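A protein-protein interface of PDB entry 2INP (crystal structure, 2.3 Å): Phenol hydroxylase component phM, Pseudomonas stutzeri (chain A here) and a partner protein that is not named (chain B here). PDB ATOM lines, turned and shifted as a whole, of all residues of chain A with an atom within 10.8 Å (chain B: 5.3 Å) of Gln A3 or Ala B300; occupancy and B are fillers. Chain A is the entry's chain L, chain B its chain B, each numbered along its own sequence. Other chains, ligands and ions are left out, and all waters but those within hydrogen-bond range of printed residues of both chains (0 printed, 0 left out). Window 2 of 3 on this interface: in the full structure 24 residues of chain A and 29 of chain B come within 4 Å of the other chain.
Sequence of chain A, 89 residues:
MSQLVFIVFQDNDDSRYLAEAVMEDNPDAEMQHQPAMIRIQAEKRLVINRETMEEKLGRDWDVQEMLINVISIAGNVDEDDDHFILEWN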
ATOM      1  N   GLN A   3     -16.420  -1.655 -16.107  1.00  0.00           N
ATOM      2  CA  GLN A   3     -15.108  -1.482 -16.795  1.00  0.00           C
ATOM      3  C   GLN A   3     -13.997  -1.862 -15.829  1.00  0.00           C
ATOM      4  O   GLN A   3     -13.884  -3.019 -15.462  1.00  0.00           O
ATOM      5  CB  GLN A   3     -14.937  -0.054 -17.335  1.00  0.00           C
ATOM      6  N   LEU A   4     -13.191  -0.891 -15.406  1.00  0.00           N
ATOM      7  CA  LEU A   4     -11.970  -1.187 -14.632  1.00  0.00           C
ATOM      8  C   LEU A   4     -12.208  -1.623 -13.167  1.00  0.00           C
ATOM      9  O   LEU A   4     -12.813  -0.883 -12.385  1.00  0.00           O
ATOM     10  CB  LEU A   4     -10.986   0.007 -14.652  1.00  0.00           C
ATOM     11  CG  LEU A   4     -10.416   0.612 -15.937  1.00  0.00           C
ATOM     12  CD1 LEU A   4     -10.897   2.053 -16.133  1.00  0.00           C
ATOM     13  CD2 LEU A   4      -8.912   0.587 -15.863  1.00  0.00           C
ATOM     14  N   VAL A   5     -11.739  -2.823 -12.803  1.00  0.00           N
ATOM     15  CA  VAL A   5     -11.613  -3.165 -11.376  1.00  0.00           C
ATOM     16  C   VAL A   5     -10.276  -2.639 -10.874  1.00  0.00           C
ATOM     17  O   VAL A   5      -9.408  -2.233 -11.656  1.00  0.00           O
ATOM     18  CB  VAL A   5     -11.794  -4.693 -11.010  1.00  0.00           C
ATOM     19  CG1 VAL A   5     -13.243  -5.133 -11.208  1.00  0.00           C
ATOM     20  CG2 VAL A   5     -10.799  -5.602 -11.743  1.00  0.00           C
ATOM     21  N   PHE A   6     -10.093  -2.610  -9.569  1.00  0.00           N
ATOM     22  CA  PHE A   6      -8.833  -2.101  -9.119  1.00  0.00           C
ATOM     23  C   PHE A   6      -8.479  -2.437  -7.690  1.00  0.00           C
ATOM     24  O   PHE A   6      -9.329  -2.741  -6.860  1.00  0.00           O
ATOM     25  CB  PHE A   6      -8.700  -0.590  -9.420  1.00  0.00           C
ATOM     26  CG  PHE A   6      -9.487   0.310  -8.486  1.00  0.00           C
ATOM     27  CD1 PHE A   6      -9.166   0.394  -7.121  1.00  0.00           C
ATOM     28  CD2 PHE A   6     -10.500   1.122  -8.980  1.00  0.00           C
ATOM     29  CE1 PHE A   6      -9.879   1.229  -6.260  1.00  0.00           C
ATOM     30  CE2 PHE A   6     -11.221   1.975  -8.122  1.00  0.00           C
ATOM     31  CZ  PHE A   6     -10.913   2.012  -6.766  1.00  0.00           C
ATOM     32  N   ILE A   7      -7.177  -2.362  -7.451  1.00  0.00           N
ATOM     33  CA  ILE A   7      -6.545  -2.677  -6.193  1.00  0.00           C
ATOM     34  C   ILE A   7      -5.317  -1.752  -6.081  1.00  0.00           C
ATOM     35  O   ILE A   7      -4.501  -1.666  -6.996  1.00  0.00           O
ATOM     36  CB  ILE A   7      -6.205  -4.222  -6.099  1.00  0.00           C
ATOM     37  CG1 ILE A   7      -5.812  -4.641  -4.664  1.00  0.00           C
ATOM     38  CG2 ILE A   7      -5.151  -4.660  -7.160  1.00  0.00           C
ATOM     39  CD1 ILE A   7      -6.093  -6.109  -4.352  1.00  0.00           C
ATOM     40  N   ASP A  28      -3.168  -8.508 -18.835  1.00  0.00           N
ATOM     41  CA  ASP A  28      -3.989  -7.451 -19.425  1.00  0.00           C
ATOM     42  C   ASP A  28      -3.995  -6.258 -18.477  1.00  0.00           C
ATOM     43  O   ASP A  28      -4.365  -5.149 -18.871  1.00  0.00           O
ATOM     44  CB  ASP A  28      -5.446  -7.897 -19.628  1.00  0.00           C
ATOM     45  CG  ASP A  28      -5.582  -9.366 -20.010  1.00  0.00           C
ATOM     46  OD1 ASP A  28      -6.681  -9.722 -20.501  1.00  0.00           O
ATOM     47  OD2 ASP A  28      -4.628 -10.167 -19.810  1.00  0.00           O
ATOM     48  N   ALA A  29      -3.599  -6.504 -17.226  1.00  0.00           N
ATOM     49  CA  ALA A  29      -3.623  -5.487 -16.174  1.00  0.00           C
ATOM     50  C   ALA A  29      -2.618  -4.387 -16.422  1.00  0.00           C
ATOM     51  O   ALA A  29      -1.493  -4.654 -16.837  1.00  0.00           O
ATOM     52  CB  ALA A  29      -3.376  -6.112 -14.813  1.00  0.00           C
ATOM     53  N   ILE A  40      -3.099  -0.756  -9.497  1.00  0.00           N
ATOM     54  CA  ILE A  40      -3.271  -1.715 -10.580  1.00  0.00           C
ATOM     55  C   ILE A  40      -4.732  -1.674 -11.091  1.00  0.00           C
ATOM     56  O   ILE A  40      -5.669  -2.062 -10.387  1.00  0.00           O
ATOM     57  CB  ILE A  40      -2.866  -3.173 -10.147  1.00  0.00           C
ATOM     58  CG1 ILE A  40      -1.512  -3.173  -9.427  1.00  0.00           C
ATOM     59  CG2 ILE A  40      -2.853  -4.147 -11.367  1.00  0.00           C
ATOM     60  CD1 ILE A  40      -0.942  -4.559  -9.156  1.00  0.00           C
ATOM     61  N   GLN A  41      -4.902  -1.171 -12.308  1.00  0.00           N
ATOM     62  CA  GLN A  41      -6.195  -1.153 -12.998  1.00  0.00           C
ATOM     63  C   GLN A  41      -6.394  -2.472 -13.759  1.00  0.00           C
ATOM     64  O   GLN A  41      -5.542  -3.368 -13.712  1.00  0.00           O
ATOM     65  CB  GLN A  41      -6.244   0.012 -14.012  1.00  0.00           C
ATOM     66  CG  GLN A  41      -6.105   1.436 -13.426  1.00  0.00           C
ATOM     67  CD  GLN A  41      -7.319   1.872 -12.610  1.00  0.00           C
ATOM     68  OE1 GLN A  41      -8.436   1.384 -12.824  1.00  0.00           O
ATOM     69  NE2 GLN A  41      -7.104   2.790 -11.660  1.00  0.00           N
ATOM     70  N   ALA A  42      -7.512  -2.574 -14.473  1.00  0.00           N
ATOM     71  CA  ALA A  42      -7.765  -3.655 -15.436  1.00  0.00           C
ATOM     72  C   ALA A  42      -9.251  -3.809 -15.709  1.00  0.00           C
ATOM     73  O   ALA A  42     -10.096  -3.520 -14.849  1.00  0.00           O
ATOM     74  CB  ALA A  42      -7.154  -4.984 -14.979  1.00  0.00           C
ATOM     75  N   GLU A  43      -9.559  -4.280 -16.913  1.00  0.00           N
ATOM     76  CA  GLU A  43     -10.931  -4.372 -17.384  1.00  0.00           C
ATOM     77  C   GLU A  43     -11.699  -5.529 -16.718  1.00  0.00           C
ATOM     78  O   GLU A  43     -11.204  -6.655 -16.637  1.00  0.00           O
ATOM     79  CB  GLU A  43     -10.925  -4.489 -18.925  1.00  0.00           C
ATOM     80  CG  GLU A  43     -12.253  -4.864 -19.598  1.00  0.00           C
ATOM     81  CD  GLU A  43     -13.331  -3.809 -19.448  1.00  0.00           C
ATOM     82  OE1 GLU A  43     -12.989  -2.664 -19.065  1.00  0.00           O
ATOM     83  OE2 GLU A  43     -14.521  -4.123 -19.714  1.00  0.00           O
ATOM     84  N   LYS A  44     -12.894  -5.229 -16.227  1.00  0.00           N
ATOM     85  CA  LYS A  44     -13.825  -6.224 -15.672  1.00  0.00           C
ATOM     86  C   LYS A  44     -13.351  -7.168 -14.525  1.00  0.00           C
ATOM     87  O   LYS A  44     -14.128  -7.435 -13.611  1.00  0.00           O
ATOM     88  CB  LYS A  44     -14.521  -7.011 -16.807  1.00  0.00           C
ATOM     89  N   ARG A  45     -12.122  -7.686 -14.566  1.00  0.00           N
ATOM     90  CA  ARG A  45     -11.642  -8.602 -13.505  1.00  0.00           C
ATOM     91  C   ARG A  45     -10.136  -8.534 -13.216  1.00  0.00           C
ATOM     92  O   ARG A  45      -9.335  -8.151 -14.068  1.00  0.00           O
ATOM     93  CB  ARG A  45     -12.059 -10.063 -13.792  1.00  0.00           C
ATOM     94  N   LEU A  46      -9.776  -8.904 -11.989  1.00  0.00           N
ATOM     95  CA  LEU A  46      -8.379  -9.050 -11.553  1.00  0.00           C
ATOM     96  C   LEU A  46      -8.255 -10.267 -10.626  1.00  0.00           C
ATOM     97  O   LEU A  46      -9.211 -10.626  -9.928  1.00  0.00           O
ATOM     98  CB  LEU A  46      -7.923  -7.806 -10.782  1.00  0.00           C
ATOM     99  CG  LEU A  46      -7.192  -6.611 -11.390  1.00  0.00           C
ATOM    100  CD1 LEU A  46      -6.884  -5.594 -10.276  1.00  0.00           C
ATOM    101  CD2 LEU A  46      -5.901  -7.025 -12.136  1.00  0.00           C
ATOM    102  N   ALA A  74     -11.769  -2.481  -5.878  1.00  0.00           N
ATOM    103  CA  ALA A  74     -12.900  -2.118  -6.741  1.00  0.00           C
ATOM    104  C   ALA A  74     -13.486  -3.312  -7.488  1.00  0.00           C
ATOM    105  O   ALA A  74     -12.761  -4.138  -8.061  1.00  0.00           O
ATOM    106  CB  ALA A  74     -12.528  -0.978  -7.707  1.00  0.00           C
ATOM    107  N   GLY A  75     -14.813  -3.396  -7.455  1.00  0.00           N
ATOM    108  CA  GLY A  75     -15.525  -4.531  -8.031  1.00  0.00           C
ATOM    109  C   GLY A  75     -15.980  -5.553  -7.007  1.00  0.00           C
ATOM    110  O   GLY A  75     -15.803  -5.378  -5.777  1.00  0.00           O
ATOM    111  N   ASN A  76     -16.567  -6.635  -7.518  1.00  0.00           N
ATOM    112  CA  ASN A  76     -17.193  -7.654  -6.665  1.00  0.00           C
ATOM    113  C   ASN A  76     -16.170  -8.625  -6.117  1.00  0.00           C
ATOM    114  O   ASN A  76     -15.370  -9.196  -6.884  1.00  0.00           O
ATOM    115  CB  ASN A  76     -18.304  -8.384  -7.428  1.00  0.00           C
ATOM    116  CG  ASN A  76     -19.476  -7.465  -7.754  1.00  0.00           C
ATOM    117  OD1 ASN A  76     -20.518  -7.521  -7.101  1.00  0.00           O
ATOM    118  ND2 ASN A  76     -19.295  -6.592  -8.740  1.00  0.00           N
ATOM    119  N   LEU A  86     -11.123  -9.620  -8.052  1.00  0.00           N
ATOM    120  CA  LEU A  86     -12.020  -8.472  -8.213  1.00  0.00           C
ATOM    121  C   LEU A  86     -12.713  -8.527  -9.599  1.00  0.00           C
ATOM    122  O   LEU A  86     -12.040  -8.680 -10.630  1.00  0.00           O
ATOM    123  CB  LEU A  86     -11.244  -7.158  -8.002  1.00  0.00           C
ATOM    124  CG  LEU A  86     -10.948  -6.772  -6.545  1.00  0.00           C
ATOM    125  CD1 LEU A  86      -9.734  -5.877  -6.436  1.00  0.00           C
ATOM    126  CD2 LEU A  86     -12.160  -6.116  -5.878  1.00  0.00           C
ATOM    127  N   GLU A  87     -14.046  -8.397  -9.619  1.00  0.00           N
ATOM    128  CA  GLU A  87     -14.830  -8.745 -10.817  1.00  0.00           C
ATOM    129  C   GLU A  87     -16.108  -7.938 -11.067  1.00  0.00           C
ATOM    130  O   GLU A  87     -16.862  -7.632 -10.145  1.00  0.00           O
ATOM    131  CB  GLU A  87     -15.163 -10.251 -10.812  1.00  0.00           C
ATOM    132  N   TRP A  88     -16.356  -7.621 -12.335  1.00  0.00           N
ATOM    133  CA  TRP A  88     -17.633  -7.040 -12.742  1.00  0.00           C
ATOM    134  C   TRP A  88     -18.486  -8.028 -13.551  1.00  0.00           C
ATOM    135  O   TRP A  88     -17.999  -8.671 -14.489  1.00  0.00           O
ATOM    136  CB  TRP A  88     -17.405  -5.751 -13.530  1.00  0.00           C
ATOM    137  CG  TRP A  88     -16.953  -4.607 -12.678  1.00  0.00           C
ATOM    138  CD1 TRP A  88     -15.831  -3.818 -12.857  1.00  0.00           C
ATOM    139  CD2 TRP A  88     -17.612  -4.098 -11.513  1.00  0.00           C
ATOM    140  NE1 TRP A  88     -15.769  -2.857 -11.873  1.00  0.00           N
ATOM    141  CE2 TRP A  88     -16.847  -3.012 -11.038  1.00  0.00           C
ATOM    142  CE3 TRP A  88     -18.782  -4.459 -10.820  1.00  0.00           C
ATOM    143  CZ2 TRP A  88     -17.221  -2.289  -9.907  1.00  0.00           C
ATOM    144  CZ3 TRP A  88     -19.147  -3.734  -9.705  1.00  0.00           C
ATOM    145  CH2 TRP A  88     -18.380  -2.665  -9.263  1.00  0.00           C
ATOM    146  N   GLU B 295     -16.682  10.169 -13.137  1.00  0.00           N
ATOM    147  CA  GLU B 295     -17.317  10.031 -14.428  1.00  0.00           C
ATOM    148  C   GLU B 295     -17.021   8.615 -14.996  1.00  0.00           C
ATOM    149  O   GLU B 295     -17.960   7.882 -15.395  1.00  0.00           O
ATOM    150  CB  GLU B 295     -16.974  11.159 -15.416  1.00  0.00           C
ATOM    151  CG  GLU B 295     -17.224  12.580 -14.894  1.00  0.00           C
ATOM    152  CD  GLU B 295     -16.806  13.646 -15.912  1.00  0.00           C
ATOM    153  OE1 GLU B 295     -16.758  14.863 -15.590  1.00  0.00           O
ATOM    154  OE2 GLU B 295     -16.499  13.248 -17.057  1.00  0.00           O
ATOM    155  N   GLN B 296     -15.749   8.209 -14.944  1.00  0.00           N
ATOM    156  CA  GLN B 296     -15.345   6.865 -15.400  1.00  0.00           C
ATOM    157  C   GLN B 296     -15.828   5.702 -14.540  1.00  0.00           C
ATOM    158  O   GLN B 296     -16.641   4.907 -15.025  1.00  0.00           O
ATOM    159  CB  GLN B 296     -13.857   6.793 -15.729  1.00  0.00           C
ATOM    160  CG  GLN B 296     -13.583   7.577 -17.007  1.00  0.00           C
ATOM    161  CD  GLN B 296     -12.206   8.259 -17.046  1.00  0.00           C
ATOM    162  OE1 GLN B 296     -11.220   7.742 -16.500  1.00  0.00           O
ATOM    163  NE2 GLN B 296     -12.144   9.424 -17.697  1.00  0.00           N
ATOM    164  N   ASN B 297     -15.380   5.603 -13.287  1.00  0.00           N
ATOM    165  CA  ASN B 297     -15.668   4.421 -12.437  1.00  0.00           C
ATOM    166  C   ASN B 297     -17.117   4.321 -12.015  1.00  0.00           C
ATOM    167  O   ASN B 297     -17.728   3.223 -11.993  1.00  0.00           O
ATOM    168  CB  ASN B 297     -14.791   4.462 -11.193  1.00  0.00           C
ATOM    169  CG  ASN B 297     -13.314   4.529 -11.539  1.00  0.00           C
ATOM    170  OD1 ASN B 297     -12.925   4.452 -12.736  1.00  0.00           O
ATOM    171  ND2 ASN B 297     -12.464   4.686 -10.503  1.00  0.00           N
ATOM    172  N   GLY B 298     -17.670   5.490 -11.677  1.00  0.00           N
ATOM    173  CA  GLY B 298     -19.056   5.612 -11.300  1.00  0.00           C
ATOM    174  C   GLY B 298     -19.942   5.342 -12.487  1.00  0.00           C
ATOM    175  O   GLY B 298     -20.910   4.634 -12.368  1.00  0.00           O
ATOM    176  N   GLY B 299     -19.605   5.920 -13.633  1.00  0.00           N
ATOM    177  CA  GLY B 299     -20.274   5.556 -14.881  1.00  0.00           C
ATOM    178  C   GLY B 299     -20.417   4.046 -15.042  1.00  0.00           C
ATOM    179  O   GLY B 299     -21.533   3.527 -15.227  1.00  0.00           O
ATOM    180  N   ALA B 300     -19.268   3.371 -14.937  1.00  0.00           N
ATOM    181  CA  ALA B 300     -19.137   1.922 -15.040  1.00  0.00           C
ATOM    182  C   ALA B 300     -20.011   1.165 -14.032  1.00  0.00           C
ATOM    183  O   ALA B 300     -20.792   0.269 -14.413  1.00  0.00           O
ATOM    184  CB  ALA B 300     -17.650   1.526 -14.880  1.00  0.00           C
ATOM    185  N   LEU B 301     -19.883   1.528 -12.754  1.00  0.00           N
ATOM    186  CA  LEU B 301     -20.678   0.928 -11.647  1.00  0.00           C
ATOM    187  C   LEU B 301     -22.221   1.039 -11.759  1.00  0.00           C
ATOM    188  O   LEU B 301     -22.931   0.087 -11.507  1.00  0.00           O
ATOM    189  CB  LEU B 301     -20.249   1.548 -10.331  1.00  0.00           C
ATOM    190  CG  LEU B 301     -21.350   1.382  -9.300  1.00  0.00           C
ATOM    191  CD1 LEU B 301     -21.274  -0.047  -8.704  1.00  0.00           C
ATOM    192  CD2 LEU B 301     -21.303   2.479  -8.240  1.00  0.00           C
ATOM    193  N   PHE B 302     -22.727   2.219 -12.090  1.00  0.00           N
ATOM    194  CA  PHE B 302     -24.153   2.397 -12.311  1.00  0.00           C
ATOM    195  C   PHE B 302     -24.637   1.635 -13.514  1.00  0.00           C
ATOM    196  O   PHE B 302     -25.763   1.159 -13.479  1.00  0.00           O
ATOM    197  CB  PHE B 302     -24.563   3.879 -12.342  1.00  0.00           C
ATOM    198  CG  PHE B 302     -24.517   4.523 -10.977  1.00  0.00           C
ATOM    199  CD1 PHE B 302     -23.396   5.270 -10.574  1.00  0.00           C
ATOM    200  CD2 PHE B 302     -25.562   4.316 -10.068  1.00  0.00           C
ATOM    201  CE1 PHE B 302     -23.338   5.804  -9.299  1.00  0.00           C
ATOM    202  CE2 PHE B 302     -25.513   4.850  -8.795  1.00  0.00           C
ATOM    203  CZ  PHE B 302     -24.398   5.579  -8.403  1.00  0.00           C
ATOM    204  N   LYS B 303     -23.793   1.499 -14.549  1.00  0.00           N
ATOM    205  CA  LYS B 303     -24.093   0.628 -15.711  1.00  0.00           C
ATOM    206  C   LYS B 303     -24.317  -0.838 -15.294  1.00  0.00           C
ATOM    207  O   LYS B 303     -25.325  -1.465 -15.726  1.00  0.00           O
ATOM    208  CB  LYS B 303     -23.066   0.750 -16.873  1.00  0.00           C
ATOM    209  CG  LYS B 303     -23.469  -0.041 -18.137  1.00  0.00           C
ATOM    210  CD  LYS B 303     -22.642   0.285 -19.391  1.00  0.00           C
ATOM    211  CE  LYS B 303     -23.462   1.063 -20.477  1.00  0.00           C
ATOM    212  NZ  LYS B 303     -22.738   1.196 -21.832  1.00  0.00           N
ATOM    213  N   ASP B 304     -23.419  -1.359 -14.452  1.00  0.00           N
ATOM    214  CA  ASP B 304     -23.632  -2.644 -13.822  1.00  0.00           C
ATOM    215  C   ASP B 304     -25.018  -2.746 -13.162  1.00  0.00           C
ATOM    216  O   ASP B 304     -25.643  -3.804 -13.183  1.00  0.00           O
ATOM    217  CB  ASP B 304     -22.532  -2.950 -12.798  1.00  0.00           C
ATOM    218  CG  ASP B 304     -22.824  -4.227 -11.948  1.00  0.00           C
ATOM    219  OD1 ASP B 304     -24.017  -4.527 -11.608  1.00  0.00           O
ATOM    220  OD2 ASP B 304     -21.843  -4.926 -11.581  1.00  0.00           O
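Among the printed residues, merely in contact across the chains: Gln A3 with Ala B300, Phe A6 with Asn B297, Trp A88 with Leu B301 and Trp A88 with Asp B304.
Of chain B, only Ala B300 comes within 4 Å of Gln A3. Of the printed residues of chain B, Phe A6 touches Asn B297. Ala A74 touches none of the printed residues of chain B. Of the printed residues of chain B, Trp A88 touches Leu B301 and Asp B304. Gln B296 touches none of the printed residues of chain A. Of the printed residues of chain A, Asn B297 touches Phe A6. No residue of chain A comes within 4 Å of Gly B298. No residue of chain A comes within 4 Å of Gly B299. Of chain A, only Trp A88 (3.9 Å) comes within 4 Å of Leu B301. The nearest residue of chain A that does not touch Ala B300 is Leu A4 (5.1 Å). The nearest printed residue of chain B that does not touch Phe A6 is Gly B298 (8.2 Å).
The backbone carbonyl oxygen (O) of Gln A3 sits at hydrogen-bond distance from the backbone NH (N) of Lys A44, 2.5 Å away. O of Phe A6 is in hydrogen-bond range of N of Ala A74, 2.6 Å away. O of Lys A44 lies within hydrogen-bond range of N of Trp A88 (2.6 Å).
Of the 20 printed residues of chain A, 3 touch a printed residue of chain B. Printed residues of chain A that touch a printed residue of chain B: Gln A3, Phe A6 and Trp A88. Hydrophobic or aromatic side chains of chain A within 4 Å of the printed part of chain B: Phe A6 and Trp A88. Of the 10 printed residues of chain B, 4 touch a printed residue of chain A. Hydrophobic or aromatic side chains of chain B that line the printed part of chain A: Ala B300 and Leu B301.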
